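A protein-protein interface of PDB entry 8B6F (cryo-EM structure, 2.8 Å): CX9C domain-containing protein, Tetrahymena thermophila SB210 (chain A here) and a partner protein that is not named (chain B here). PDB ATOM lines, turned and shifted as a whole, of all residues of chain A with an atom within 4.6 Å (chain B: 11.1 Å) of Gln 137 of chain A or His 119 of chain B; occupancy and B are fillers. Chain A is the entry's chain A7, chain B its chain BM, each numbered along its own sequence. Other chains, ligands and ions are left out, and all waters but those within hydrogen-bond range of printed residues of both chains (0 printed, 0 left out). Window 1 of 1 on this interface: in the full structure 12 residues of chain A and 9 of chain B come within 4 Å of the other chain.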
ATOM      1  N   GLU A 133      37.787 -18.389 -32.921  1.00  0.00           N
ATOM      2  CA  GLU A 133      36.436 -18.771 -32.523  1.00  0.00           C
ATOM      3  C   GLU A 133      35.836 -19.774 -33.501  1.00  0.00           C
ATOM      4  O   GLU A 133      35.245 -20.778 -33.092  1.00  0.00           O
ATOM      5  CB  GLU A 133      35.552 -17.531 -32.409  1.00  0.00           C
ATOM      6  CG  GLU A 133      35.916 -16.643 -31.232  1.00  0.00           C
ATOM      7  CD  GLU A 133      35.053 -15.404 -31.152  1.00  0.00           C
ATOM      8  OE1 GLU A 133      34.091 -15.295 -31.939  1.00  0.00           O
ATOM      9  OE2 GLU A 133      35.336 -14.534 -30.301  1.00  0.00           O
ATOM     10  N   ASP A 134      35.984 -19.520 -34.802  1.00  0.00           N
ATOM     11  CA  ASP A 134      35.468 -20.449 -35.802  1.00  0.00           C
ATOM     12  C   ASP A 134      36.122 -21.817 -35.680  1.00  0.00           C
ATOM     13  O   ASP A 134      35.451 -22.847 -35.799  1.00  0.00           O
ATOM     14  CB  ASP A 134      35.688 -19.887 -37.205  1.00  0.00           C
ATOM     15  CG  ASP A 134      34.732 -18.767 -37.542  1.00  0.00           C
ATOM     16  OD1 ASP A 134      34.774 -17.722 -36.862  1.00  0.00           O
ATOM     17  OD2 ASP A 134      33.938 -18.930 -38.490  1.00  0.00           O
ATOM     18  N   CYS A 135      37.433 -21.848 -35.443  1.00  0.00           N
ATOM     19  CA  CYS A 135      38.124 -23.123 -35.295  1.00  0.00           C
ATOM     20  C   CYS A 135      37.606 -23.901 -34.090  1.00  0.00           C
ATOM     21  O   CYS A 135      37.428 -25.122 -34.163  1.00  0.00           O
ATOM     22  CB  CYS A 135      39.629 -22.884 -35.185  1.00  0.00           C
ATOM     23  SG  CYS A 135      40.626 -24.373 -35.349  1.00  0.00           S
ATOM     24  N   ARG A 136      37.359 -23.216 -32.973  1.00  0.00           N
ATOM     25  CA  ARG A 136      36.931 -23.887 -31.751  1.00  0.00           C
ATOM     26  C   ARG A 136      35.436 -24.177 -31.707  1.00  0.00           C
ATOM     27  O   ARG A 136      34.987 -24.856 -30.778  1.00  0.00           O
ATOM     28  CB  ARG A 136      37.312 -23.048 -30.527  1.00  0.00           C
ATOM     29  CG  ARG A 136      36.624 -21.696 -30.475  1.00  0.00           C
ATOM     30  CD  ARG A 136      37.007 -20.901 -29.238  1.00  0.00           C
ATOM     31  NE  ARG A 136      36.319 -21.389 -28.049  1.00  0.00           N
ATOM     32  CZ  ARG A 136      36.798 -22.302 -27.216  1.00  0.00           C
ATOM     33  NH1 ARG A 136      37.984 -22.859 -27.404  1.00  0.00           N
ATOM     34  NH2 ARG A 136      36.067 -22.670 -26.168  1.00  0.00           N
ATOM     35  N   GLN A 137      34.656 -23.685 -32.667  1.00  0.00           N
ATOM     36  CA  GLN A 137      33.218 -23.927 -32.654  1.00  0.00           C
ATOM     37  C   GLN A 137      32.919 -25.421 -32.674  1.00  0.00           C
ATOM     38  O   GLN A 137      33.602 -26.202 -33.343  1.00  0.00           O
ATOM     39  CB  GLN A 137      32.558 -23.242 -33.851  1.00  0.00           C
ATOM     40  CG  GLN A 137      32.234 -21.770 -33.635  1.00  0.00           C
ATOM     41  CD  GLN A 137      31.075 -21.554 -32.687  1.00  0.00           C
ATOM     42  OE1 GLN A 137      30.614 -22.484 -32.029  1.00  0.00           O
ATOM     43  NE2 GLN A 137      30.589 -20.321 -32.620  1.00  0.00           N
ATOM     44  N   THR A 138      31.884 -25.817 -31.933  1.00  0.00           N
ATOM     45  CA  THR A 138      31.490 -27.212 -31.811  1.00  0.00           C
ATOM     46  C   THR A 138      29.972 -27.284 -31.707  1.00  0.00           C
ATOM     47  O   THR A 138      29.302 -26.287 -31.431  1.00  0.00           O
ATOM     48  CB  THR A 138      32.146 -27.873 -30.585  1.00  0.00           C
ATOM     49  OG1 THR A 138      33.542 -27.561 -30.563  1.00  0.00           O
ATOM     50  CG2 THR A 138      31.988 -29.385 -30.614  1.00  0.00           C
ATOM     51  N   THR A 140      28.317 -29.025 -29.498  1.00  0.00           N
ATOM     52  CA  THR A 140      27.929 -29.235 -28.113  1.00  0.00           C
ATOM     53  C   THR A 140      28.706 -28.277 -27.226  1.00  0.00           C
ATOM     54  O   THR A 140      29.781 -27.802 -27.604  1.00  0.00           O
ATOM     55  CB  THR A 140      28.200 -30.681 -27.669  1.00  0.00           C
ATOM     56  OG1 THR A 140      29.586 -30.991 -27.861  1.00  0.00           O
ATOM     57  CG2 THR A 140      27.355 -31.652 -28.469  1.00  0.00           C
ATOM     58  N   PRO A 141      28.187 -27.970 -26.036  1.00  0.00           N
ATOM     59  CA  PRO A 141      28.920 -27.067 -25.134  1.00  0.00           C
ATOM     60  C   PRO A 141      30.258 -27.615 -24.678  1.00  0.00           C
ATOM     61  O   PRO A 141      31.099 -26.838 -24.212  1.00  0.00           O
ATOM     62  CB  PRO A 141      27.955 -26.887 -23.953  1.00  0.00           C
ATOM     63  CG  PRO A 141      27.093 -28.078 -23.992  1.00  0.00           C
ATOM     64  CD  PRO A 141      26.923 -28.428 -25.436  1.00  0.00           C
ATOM     65  N   LEU A 142      30.482 -28.920 -24.786  1.00  0.00           N
ATOM     66  CA  LEU A 142      31.763 -29.477 -24.388  1.00  0.00           C
ATOM     67  C   LEU A 142      32.875 -28.871 -25.240  1.00  0.00           C
ATOM     68  O   LEU A 142      32.724 -28.746 -26.461  1.00  0.00           O
ATOM     69  CB  LEU A 142      31.760 -30.999 -24.537  1.00  0.00           C
ATOM     70  CG  LEU A 142      30.774 -31.764 -23.654  1.00  0.00           C
ATOM     71  CD1 LEU A 142      30.822 -33.243 -23.977  1.00  0.00           C
ATOM     72  CD2 LEU A 142      31.062 -31.536 -22.178  1.00  0.00           C
ATOM     73  N   PRO A 143      34.003 -28.497 -24.642  1.00  0.00           N
ATOM     74  CA  PRO A 143      35.053 -27.820 -25.407  1.00  0.00           C
ATOM     75  C   PRO A 143      35.691 -28.739 -26.435  1.00  0.00           C
ATOM     76  O   PRO A 143      35.682 -29.965 -26.319  1.00  0.00           O
ATOM     77  CB  PRO A 143      36.063 -27.401 -24.334  1.00  0.00           C
ATOM     78  CG  PRO A 143      35.855 -28.362 -23.231  1.00  0.00           C
ATOM     79  CD  PRO A 143      34.392 -28.689 -23.234  1.00  0.00           C
ATOM     80  N   LYS A 144      36.242 -28.113 -27.467  1.00  0.00           N
ATOM     81  CA  LYS A 144      36.961 -28.813 -28.518  1.00  0.00           C
ATOM     82  C   LYS A 144      38.423 -28.989 -28.120  1.00  0.00           C
ATOM     83  O   LYS A 144      38.964 -28.248 -27.297  1.00  0.00           O
ATOM     84  CB  LYS A 144      36.858 -28.042 -29.834  1.00  0.00           C
ATOM     85  CG  LYS A 144      37.311 -28.812 -31.059  1.00  0.00           C
ATOM     86  CD  LYS A 144      37.023 -28.025 -32.327  1.00  0.00           C
ATOM     87  CE  LYS A 144      37.403 -28.810 -33.567  1.00  0.00           C
ATOM     88  NZ  LYS A 144      37.076 -28.064 -34.814  1.00  0.00           N
ATOM     89  N   PHE B  99      21.968 -22.163 -20.056  1.00  0.00           N
ATOM     90  CA  PHE B  99      22.362 -22.907 -21.248  1.00  0.00           C
ATOM     91  C   PHE B  99      22.488 -24.395 -20.953  1.00  0.00           C
ATOM     92  O   PHE B  99      22.117 -25.234 -21.782  1.00  0.00           O
ATOM     93  CB  PHE B  99      23.674 -22.359 -21.808  1.00  0.00           C
ATOM     94  CG  PHE B  99      24.877 -22.711 -20.988  1.00  0.00           C
ATOM     95  CD1 PHE B  99      25.219 -21.961 -19.878  1.00  0.00           C
ATOM     96  CD2 PHE B  99      25.673 -23.791 -21.332  1.00  0.00           C
ATOM     97  CE1 PHE B  99      26.327 -22.284 -19.123  1.00  0.00           C
ATOM     98  CE2 PHE B  99      26.782 -24.120 -20.581  1.00  0.00           C
ATOM     99  CZ  PHE B  99      27.111 -23.365 -19.475  1.00  0.00           C
ATOM    100  N   GLY B 100      23.017 -24.748 -19.783  1.00  0.00           N
ATOM    101  CA  GLY B 100      23.109 -26.152 -19.424  1.00  0.00           C
ATOM    102  C   GLY B 100      21.754 -26.831 -19.420  1.00  0.00           C
ATOM    103  O   GLY B 100      21.608 -27.951 -19.912  1.00  0.00           O
ATOM    104  N   THR B 102      18.977 -25.712 -21.101  1.00  0.00           N
ATOM    105  CA  THR B 102      18.297 -25.660 -22.391  1.00  0.00           C
ATOM    106  C   THR B 102      18.901 -26.649 -23.382  1.00  0.00           C
ATOM    107  O   THR B 102      18.171 -27.268 -24.164  1.00  0.00           O
ATOM    108  CB  THR B 102      18.331 -24.233 -22.949  1.00  0.00           C
ATOM    109  OG1 THR B 102      17.361 -24.105 -23.994  1.00  0.00           O
ATOM    110  CG2 THR B 102      19.693 -23.894 -23.523  1.00  0.00           C
ATOM    111  N   PHE B 103      20.227 -26.805 -23.380  1.00  0.00           N
ATOM    112  CA  PHE B 103      20.847 -27.727 -24.326  1.00  0.00           C
ATOM    113  C   PHE B 103      20.357 -29.151 -24.115  1.00  0.00           C
ATOM    114  O   PHE B 103      19.934 -29.822 -25.062  1.00  0.00           O
ATOM    115  CB  PHE B 103      22.369 -27.680 -24.204  1.00  0.00           C
ATOM    116  CG  PHE B 103      23.060 -28.712 -25.043  1.00  0.00           C
ATOM    117  CD1 PHE B 103      23.286 -28.489 -26.389  1.00  0.00           C
ATOM    118  CD2 PHE B 103      23.462 -29.916 -24.491  1.00  0.00           C
ATOM    119  CE1 PHE B 103      23.908 -29.440 -27.168  1.00  0.00           C
ATOM    120  CE2 PHE B 103      24.086 -30.873 -25.264  1.00  0.00           C
ATOM    121  CZ  PHE B 103      24.310 -30.634 -26.605  1.00  0.00           C
ATOM    122  N   GLY B 115      17.743 -26.306 -33.537  1.00  0.00           N
ATOM    123  CA  GLY B 115      18.793 -26.327 -34.538  1.00  0.00           C
ATOM    124  C   GLY B 115      20.169 -26.586 -33.963  1.00  0.00           C
ATOM    125  O   GLY B 115      20.299 -27.215 -32.909  1.00  0.00           O
ATOM    126  N   ARG B 116      21.207 -26.108 -34.645  1.00  0.00           N
ATOM    127  CA  ARG B 116      22.569 -26.317 -34.182  1.00  0.00           C
ATOM    128  C   ARG B 116      22.859 -25.448 -32.964  1.00  0.00           C
ATOM    129  O   ARG B 116      22.153 -24.478 -32.675  1.00  0.00           O
ATOM    130  CB  ARG B 116      23.571 -26.011 -35.294  1.00  0.00           C
ATOM    131  CG  ARG B 116      23.474 -26.947 -36.487  1.00  0.00           C
ATOM    132  CD  ARG B 116      24.561 -26.651 -37.506  1.00  0.00           C
ATOM    133  NE  ARG B 116      24.484 -25.279 -37.991  1.00  0.00           N
ATOM    134  CZ  ARG B 116      25.383 -24.710 -38.782  1.00  0.00           C
ATOM    135  NH1 ARG B 116      26.455 -25.366 -39.195  1.00  0.00           N
ATOM    136  NH2 ARG B 116      25.203 -23.451 -39.168  1.00  0.00           N
ATOM    137  N   TRP B 117      23.920 -25.803 -32.247  1.00  0.00           N
ATOM    138  CA  TRP B 117      24.284 -25.158 -30.994  1.00  0.00           C
ATOM    139  C   TRP B 117      25.502 -24.272 -31.212  1.00  0.00           C
ATOM    140  O   TRP B 117      26.503 -24.713 -31.784  1.00  0.00           O
ATOM    141  CB  TRP B 117      24.575 -26.199 -29.910  1.00  0.00           C
ATOM    142  CG  TRP B 117      24.972 -25.615 -28.586  1.00  0.00           C
ATOM    143  CD1 TRP B 117      26.240 -25.389 -28.138  1.00  0.00           C
ATOM    144  CD2 TRP B 117      24.094 -25.190 -27.536  1.00  0.00           C
ATOM    145  NE1 TRP B 117      26.207 -24.848 -26.876  1.00  0.00           N
ATOM    146  CE2 TRP B 117      24.901 -24.716 -26.484  1.00  0.00           C
ATOM    147  CE3 TRP B 117      22.705 -25.163 -27.386  1.00  0.00           C
ATOM    148  CZ2 TRP B 117      24.364 -24.221 -25.299  1.00  0.00           C
ATOM    149  CZ3 TRP B 117      22.173 -24.672 -26.206  1.00  0.00           C
ATOM    150  CH2 TRP B 117      23.002 -24.207 -25.178  1.00  0.00           C
ATOM    151  N   ASN B 118      25.411 -23.027 -30.753  1.00  0.00           N
ATOM    152  CA  ASN B 118      26.528 -22.091 -30.822  1.00  0.00           C
ATOM    153  C   ASN B 118      27.427 -22.336 -29.617  1.00  0.00           C
ATOM    154  O   ASN B 118      27.072 -21.987 -28.487  1.00  0.00           O
ATOM    155  CB  ASN B 118      26.012 -20.656 -30.850  1.00  0.00           C
ATOM    156  CG  ASN B 118      26.932 -19.723 -31.599  1.00  0.00           C
ATOM    157  OD1 ASN B 118      27.992 -19.350 -31.105  1.00  0.00           O
ATOM    158  ND2 ASN B 118      26.523 -19.326 -32.797  1.00  0.00           N
ATOM    159  N   HIS B 119      28.595 -22.938 -29.852  1.00  0.00           N
ATOM    160  CA  HIS B 119      29.433 -23.383 -28.744  1.00  0.00           C
ATOM    161  C   HIS B 119      29.926 -22.209 -27.907  1.00  0.00           C
ATOM    162  O   HIS B 119      29.772 -22.200 -26.680  1.00  0.00           O
ATOM    163  CB  HIS B 119      30.615 -24.189 -29.275  1.00  0.00           C
ATOM    164  CG  HIS B 119      31.661 -24.468 -28.245  1.00  0.00           C
ATOM    165  ND1 HIS B 119      31.411 -25.214 -27.113  1.00  0.00           N
ATOM    166  CD2 HIS B 119      32.960 -24.095 -28.170  1.00  0.00           C
ATOM    167  CE1 HIS B 119      32.512 -25.289 -26.388  1.00  0.00           C
ATOM    168  NE2 HIS B 119      33.467 -24.619 -27.007  1.00  0.00           N
ATOM    169  N   ASN B 120      30.520 -21.207 -28.550  1.00  0.00           N
ATOM    170  CA  ASN B 120      31.144 -20.116 -27.811  1.00  0.00           C
ATOM    171  C   ASN B 120      30.140 -19.102 -27.285  1.00  0.00           C
ATOM    172  O   ASN B 120      30.528 -18.222 -26.511  1.00  0.00           O
ATOM    173  CB  ASN B 120      32.185 -19.412 -28.684  1.00  0.00           C
ATOM    174  CG  ASN B 120      31.635 -18.996 -30.027  1.00  0.00           C
ATOM    175  OD1 ASN B 120      30.424 -18.927 -30.221  1.00  0.00           O
ATOM    176  ND2 ASN B 120      32.527 -18.714 -30.968  1.00  0.00           N
ATOM    177  N   PHE B 121      28.870 -19.195 -27.683  1.00  0.00           N
ATOM    178  CA  PHE B 121      27.824 -18.347 -27.134  1.00  0.00           C
ATOM    179  C   PHE B 121      26.749 -19.120 -26.388  1.00  0.00           C
ATOM    180  O   PHE B 121      25.867 -18.492 -25.791  1.00  0.00           O
ATOM    181  CB  PHE B 121      27.168 -17.514 -28.247  1.00  0.00           C
ATOM    182  CG  PHE B 121      28.037 -16.401 -28.749  1.00  0.00           C
ATOM    183  CD1 PHE B 121      28.227 -15.261 -27.988  1.00  0.00           C
ATOM    184  CD2 PHE B 121      28.671 -16.498 -29.975  1.00  0.00           C
ATOM    185  CE1 PHE B 121      29.030 -14.235 -28.441  1.00  0.00           C
ATOM    186  CE2 PHE B 121      29.476 -15.476 -30.435  1.00  0.00           C
ATOM    187  CZ  PHE B 121      29.656 -14.341 -29.667  1.00  0.00           C
ATOM    188  N   ALA B 122      26.795 -20.450 -26.398  1.00  0.00           N
ATOM    189  CA  ALA B 122      25.923 -21.282 -25.576  1.00  0.00           C
ATOM    190  C   ALA B 122      24.448 -20.987 -25.847  1.00  0.00           C
ATOM    191  O   ALA B 122      23.696 -20.562 -24.967  1.00  0.00           O
ATOM    192  CB  ALA B 122      26.255 -21.100 -24.091  1.00  0.00           C
ATOM    193  N   CYS B 123      24.041 -21.224 -27.090  1.00  0.00           N
ATOM    194  CA  CYS B 123      22.644 -21.066 -27.473  1.00  0.00           C
ATOM    195  C   CYS B 123      22.436 -21.702 -28.836  1.00  0.00           C
ATOM    196  O   CYS B 123      23.389 -21.930 -29.587  1.00  0.00           O
ATOM    197  CB  CYS B 123      22.227 -19.593 -27.499  1.00  0.00           C
ATOM    198  SG  CYS B 123      23.387 -18.504 -28.346  1.00  0.00           S
ATOM    199  N   TYR B 124      21.175 -21.987 -29.144  1.00  0.00           N
ATOM    200  CA  TYR B 124      20.819 -22.555 -30.432  1.00  0.00           C
ATOM    201  C   TYR B 124      20.658 -21.454 -31.476  1.00  0.00           C
ATOM    202  O   TYR B 124      20.512 -20.273 -31.157  1.00  0.00           O
ATOM    203  CB  TYR B 124      19.526 -23.362 -30.331  1.00  0.00           C
ATOM    204  CG  TYR B 124      19.666 -24.671 -29.589  1.00  0.00           C
ATOM    205  CD1 TYR B 124      20.187 -25.793 -30.219  1.00  0.00           C
ATOM    206  CD2 TYR B 124      19.266 -24.789 -28.267  1.00  0.00           C
ATOM    207  CE1 TYR B 124      20.309 -26.993 -29.553  1.00  0.00           C
ATOM    208  CE2 TYR B 124      19.386 -25.987 -27.591  1.00  0.00           C
ATOM    209  CZ  TYR B 124      19.907 -27.085 -28.241  1.00  0.00           C
ATOM    210  OH  TYR B 124      20.030 -28.283 -27.579  1.00  0.00           O
ATOM    211  N   GLU B 125      20.685 -21.864 -32.744  1.00  0.00           N
ATOM    212  CA  GLU B 125      20.567 -20.899 -33.831  1.00  0.00           C
ATOM    213  C   GLU B 125      19.235 -20.163 -33.780  1.00  0.00           C
ATOM    214  O   GLU B 125      19.184 -18.943 -33.977  1.00  0.00           O
ATOM    215  CB  GLU B 125      20.731 -21.600 -35.179  1.00  0.00           C
ATOM    216  CG  GLU B 125      22.147 -22.055 -35.476  1.00  0.00           C
ATOM    217  CD  GLU B 125      22.260 -22.749 -36.820  1.00  0.00           C
ATOM    218  OE1 GLU B 125      21.247 -23.307 -37.289  1.00  0.00           O
ATOM    219  OE2 GLU B 125      23.360 -22.729 -37.412  1.00  0.00           O
ATOM    220  N   GLN B 127      17.167 -19.588 -31.286  1.00  0.00           N
ATOM    221  CA  GLN B 127      16.867 -18.755 -30.132  1.00  0.00           C
ATOM    222  C   GLN B 127      17.118 -17.287 -30.477  1.00  0.00           C
ATOM    223  O   GLN B 127      18.099 -16.970 -31.156  1.00  0.00           O
ATOM    224  CB  GLN B 127      17.716 -19.164 -28.931  1.00  0.00           C
ATOM    225  CG  GLN B 127      17.288 -20.477 -28.291  1.00  0.00           C
ATOM    226  CD  GLN B 127      18.098 -20.816 -27.055  1.00  0.00           C
ATOM    227  OE1 GLN B 127      19.031 -20.102 -26.694  1.00  0.00           O
ATOM    228  NE2 GLN B 127      17.742 -21.913 -26.397  1.00  0.00           N
ATOM    229  N   CYS B 130      20.917 -15.248 -30.480  1.00  0.00           N
ATOM    230  CA  CYS B 130      21.848 -16.230 -29.938  1.00  0.00           C
ATOM    231  C   CYS B 130      23.278 -15.705 -29.967  1.00  0.00           C
ATOM    232  O   CYS B 130      23.904 -15.508 -28.920  1.00  0.00           O
ATOM    233  CB  CYS B 130      21.731 -17.543 -30.716  1.00  0.00           C
ATOM    234  SG  CYS B 130      23.010 -18.765 -30.327  1.00  0.00           S
ATOM    235  N   GLY B 131      23.809 -15.462 -31.162  1.00  0.00           N
ATOM    236  CA  GLY B 131      25.152 -14.933 -31.284  1.00  0.00           C
ATOM    237  C   GLY B 131      25.162 -13.428 -31.424  1.00  0.00           C
ATOM    238  O   GLY B 131      24.994 -12.904 -32.527  1.00  0.00           O
ATOM    239  N   ARG B 132      25.373 -12.720 -30.318  1.00  0.00           N
ATOM    240  CA  ARG B 132      25.368 -11.262 -30.296  1.00  0.00           C
ATOM    241  C   ARG B 132      26.792 -10.791 -30.034  1.00  0.00           C
ATOM    242  O   ARG B 132      27.309 -10.948 -28.923  1.00  0.00           O
ATOM    243  CB  ARG B 132      24.406 -10.738 -29.232  1.00  0.00           C
ATOM    244  CG  ARG B 132      23.835  -9.359 -29.524  1.00  0.00           C
ATOM    245  CD  ARG B 132      23.017  -9.365 -30.802  1.00  0.00           C
ATOM    246  NE  ARG B 132      22.190  -8.174 -30.947  1.00  0.00           N
ATOM    247  CZ  ARG B 132      20.949  -8.059 -30.494  1.00  0.00           C
ATOM    248  NH1 ARG B 132      20.363  -9.038 -29.823  1.00  0.00           N
ATOM    249  NH2 ARG B 132      20.276  -6.937 -30.725  1.00  0.00           N
ATOM    250  N   ASP B 133      27.418 -10.213 -31.053  1.00  0.00           N
ATOM    251  CA  ASP B 133      28.810  -9.804 -30.992  1.00  0.00           C
ATOM    252  C   ASP B 133      28.913  -8.294 -31.146  1.00  0.00           C
ATOM    253  O   ASP B 133      27.996  -7.634 -31.642  1.00  0.00           O
ATOM    254  CB  ASP B 133      29.632 -10.503 -32.080  1.00  0.00           C
ATOM    255  CG  ASP B 133      30.978 -10.978 -31.579  1.00  0.00           C
ATOM    256  OD1 ASP B 133      31.553 -10.312 -30.693  1.00  0.00           O
ATOM    257  OD2 ASP B 133      31.458 -12.021 -32.067  1.00  0.00           O
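Asn 120 of chain B touches Glu 133 of chain A (ND2 to CB, 3.6 Å). CB of His 119 of chain B touches O of Thr 138 of chain A (3.3 Å). Thr 140 of chain A touches Phe 103 of chain B (CG2 to CZ, 3.7 Å). CD1 of Trp 117 of chain B touches C of Thr 140 of chain A, 3.9 Å away. Phe 103 of chain B touches Pro 141 of chain A (CZ to CD, 3.6 Å). Trp 117 of chain B touches Pro 141 of chain A. Leu 142 of chain A touches His 119 of chain B (O to CE1, 3.5 Å). Pro 143 of chain A touches His 119 of chain B.
OH of Tyr 124 of chain B is in hydrogen-bond range of O of Phe 103 of chain B (3.0 Å). The side-chain amide oxygen (OD1) of Asn 118 of chain B sits close to the side-chain amide oxygen (OD1) of Asn 120 of chain B (2.6 Å). The backbone NH of Asn 118 of chain B is in hydrogen-bond range of the backbone carbonyl oxygen of Cys 123 of chain B. O of Arg 136 of chain A sits at hydrogen-bond distance from OG1 of Thr 138 of chain A (3.1 Å). The side-chain sulfur (SG) of Cys 123 of chain B is disulfide-bonded to the side-chain sulfur (SG) of Cys 130 of chain B (2.0 Å).
Of the 20 printed residues of chain B, 5 touch a printed residue of chain A.
Gln 137 of chain A touches just these residues of chain B: Asn 118, His 119 and Asn 120. Of chain A, only Arg 136, Gln 137, Thr 138, Thr 140, Pro 141, Leu 142 and Pro 143 come within 4 Å of His 119 of chain B. No residue of chain B comes within 4 Å of Cys 135 of chain A. Thr 138 of chain A touches just these residues of chain B: Trp 117 and His 119. Of the printed residues of chain B, Pro 141 of chain A touches Phe 103 (3.6 Å), Trp 117 (3.8 Å) and His 119 (3.0 Å). No residue of chain B comes within 4 Å of Lys 144 of chain A. Printed residues of chain A within 4 Å of Phe 103 of chain B: Thr 140 (3.7 Å) and Pro 141 (3.6 Å). Printed residues of chain B within 4 Å of Glu 133 of chain A: Asn 120. Printed residues of chain A within 4 Å of Asn 120 of chain B: Glu 133 and Gln 137. Printed residues of chain B within 4 Å of Leu 142 of chain A: His 119. The nearest residue of chain B that does not touch Gln 137 of chain A is Trp 117 of chain B (4.7 Å).
OD1 of Asn 118 of chain B is in hydrogen-bond range of NE2 of Gln 137 of chain A. NE2 of His 119 of chain B lies within hydrogen-bond range of NH2 of Arg 136 of chain A, at 3.4 Å. The backbone NH (N) of His 119 of chain B lies within hydrogen-bond range of the side-chain amide oxygen (OE1) of Gln 137 of chain A (3.0 Å). ND1 of His 119 of chain B lies within hydrogen-bond range of O of Thr 140 of chain A (3.1 Å). ND1 of His 119 of chain B lies close to O of Pro 141 of chain A, at 3.3 Å. OD1 of Asn 120 of chain B is in hydrogen-bond range of NE2 of Gln 137 of chain A (2.8 Å). O of Thr 138 of chain A sits close to O of Trp 117 of chain B.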
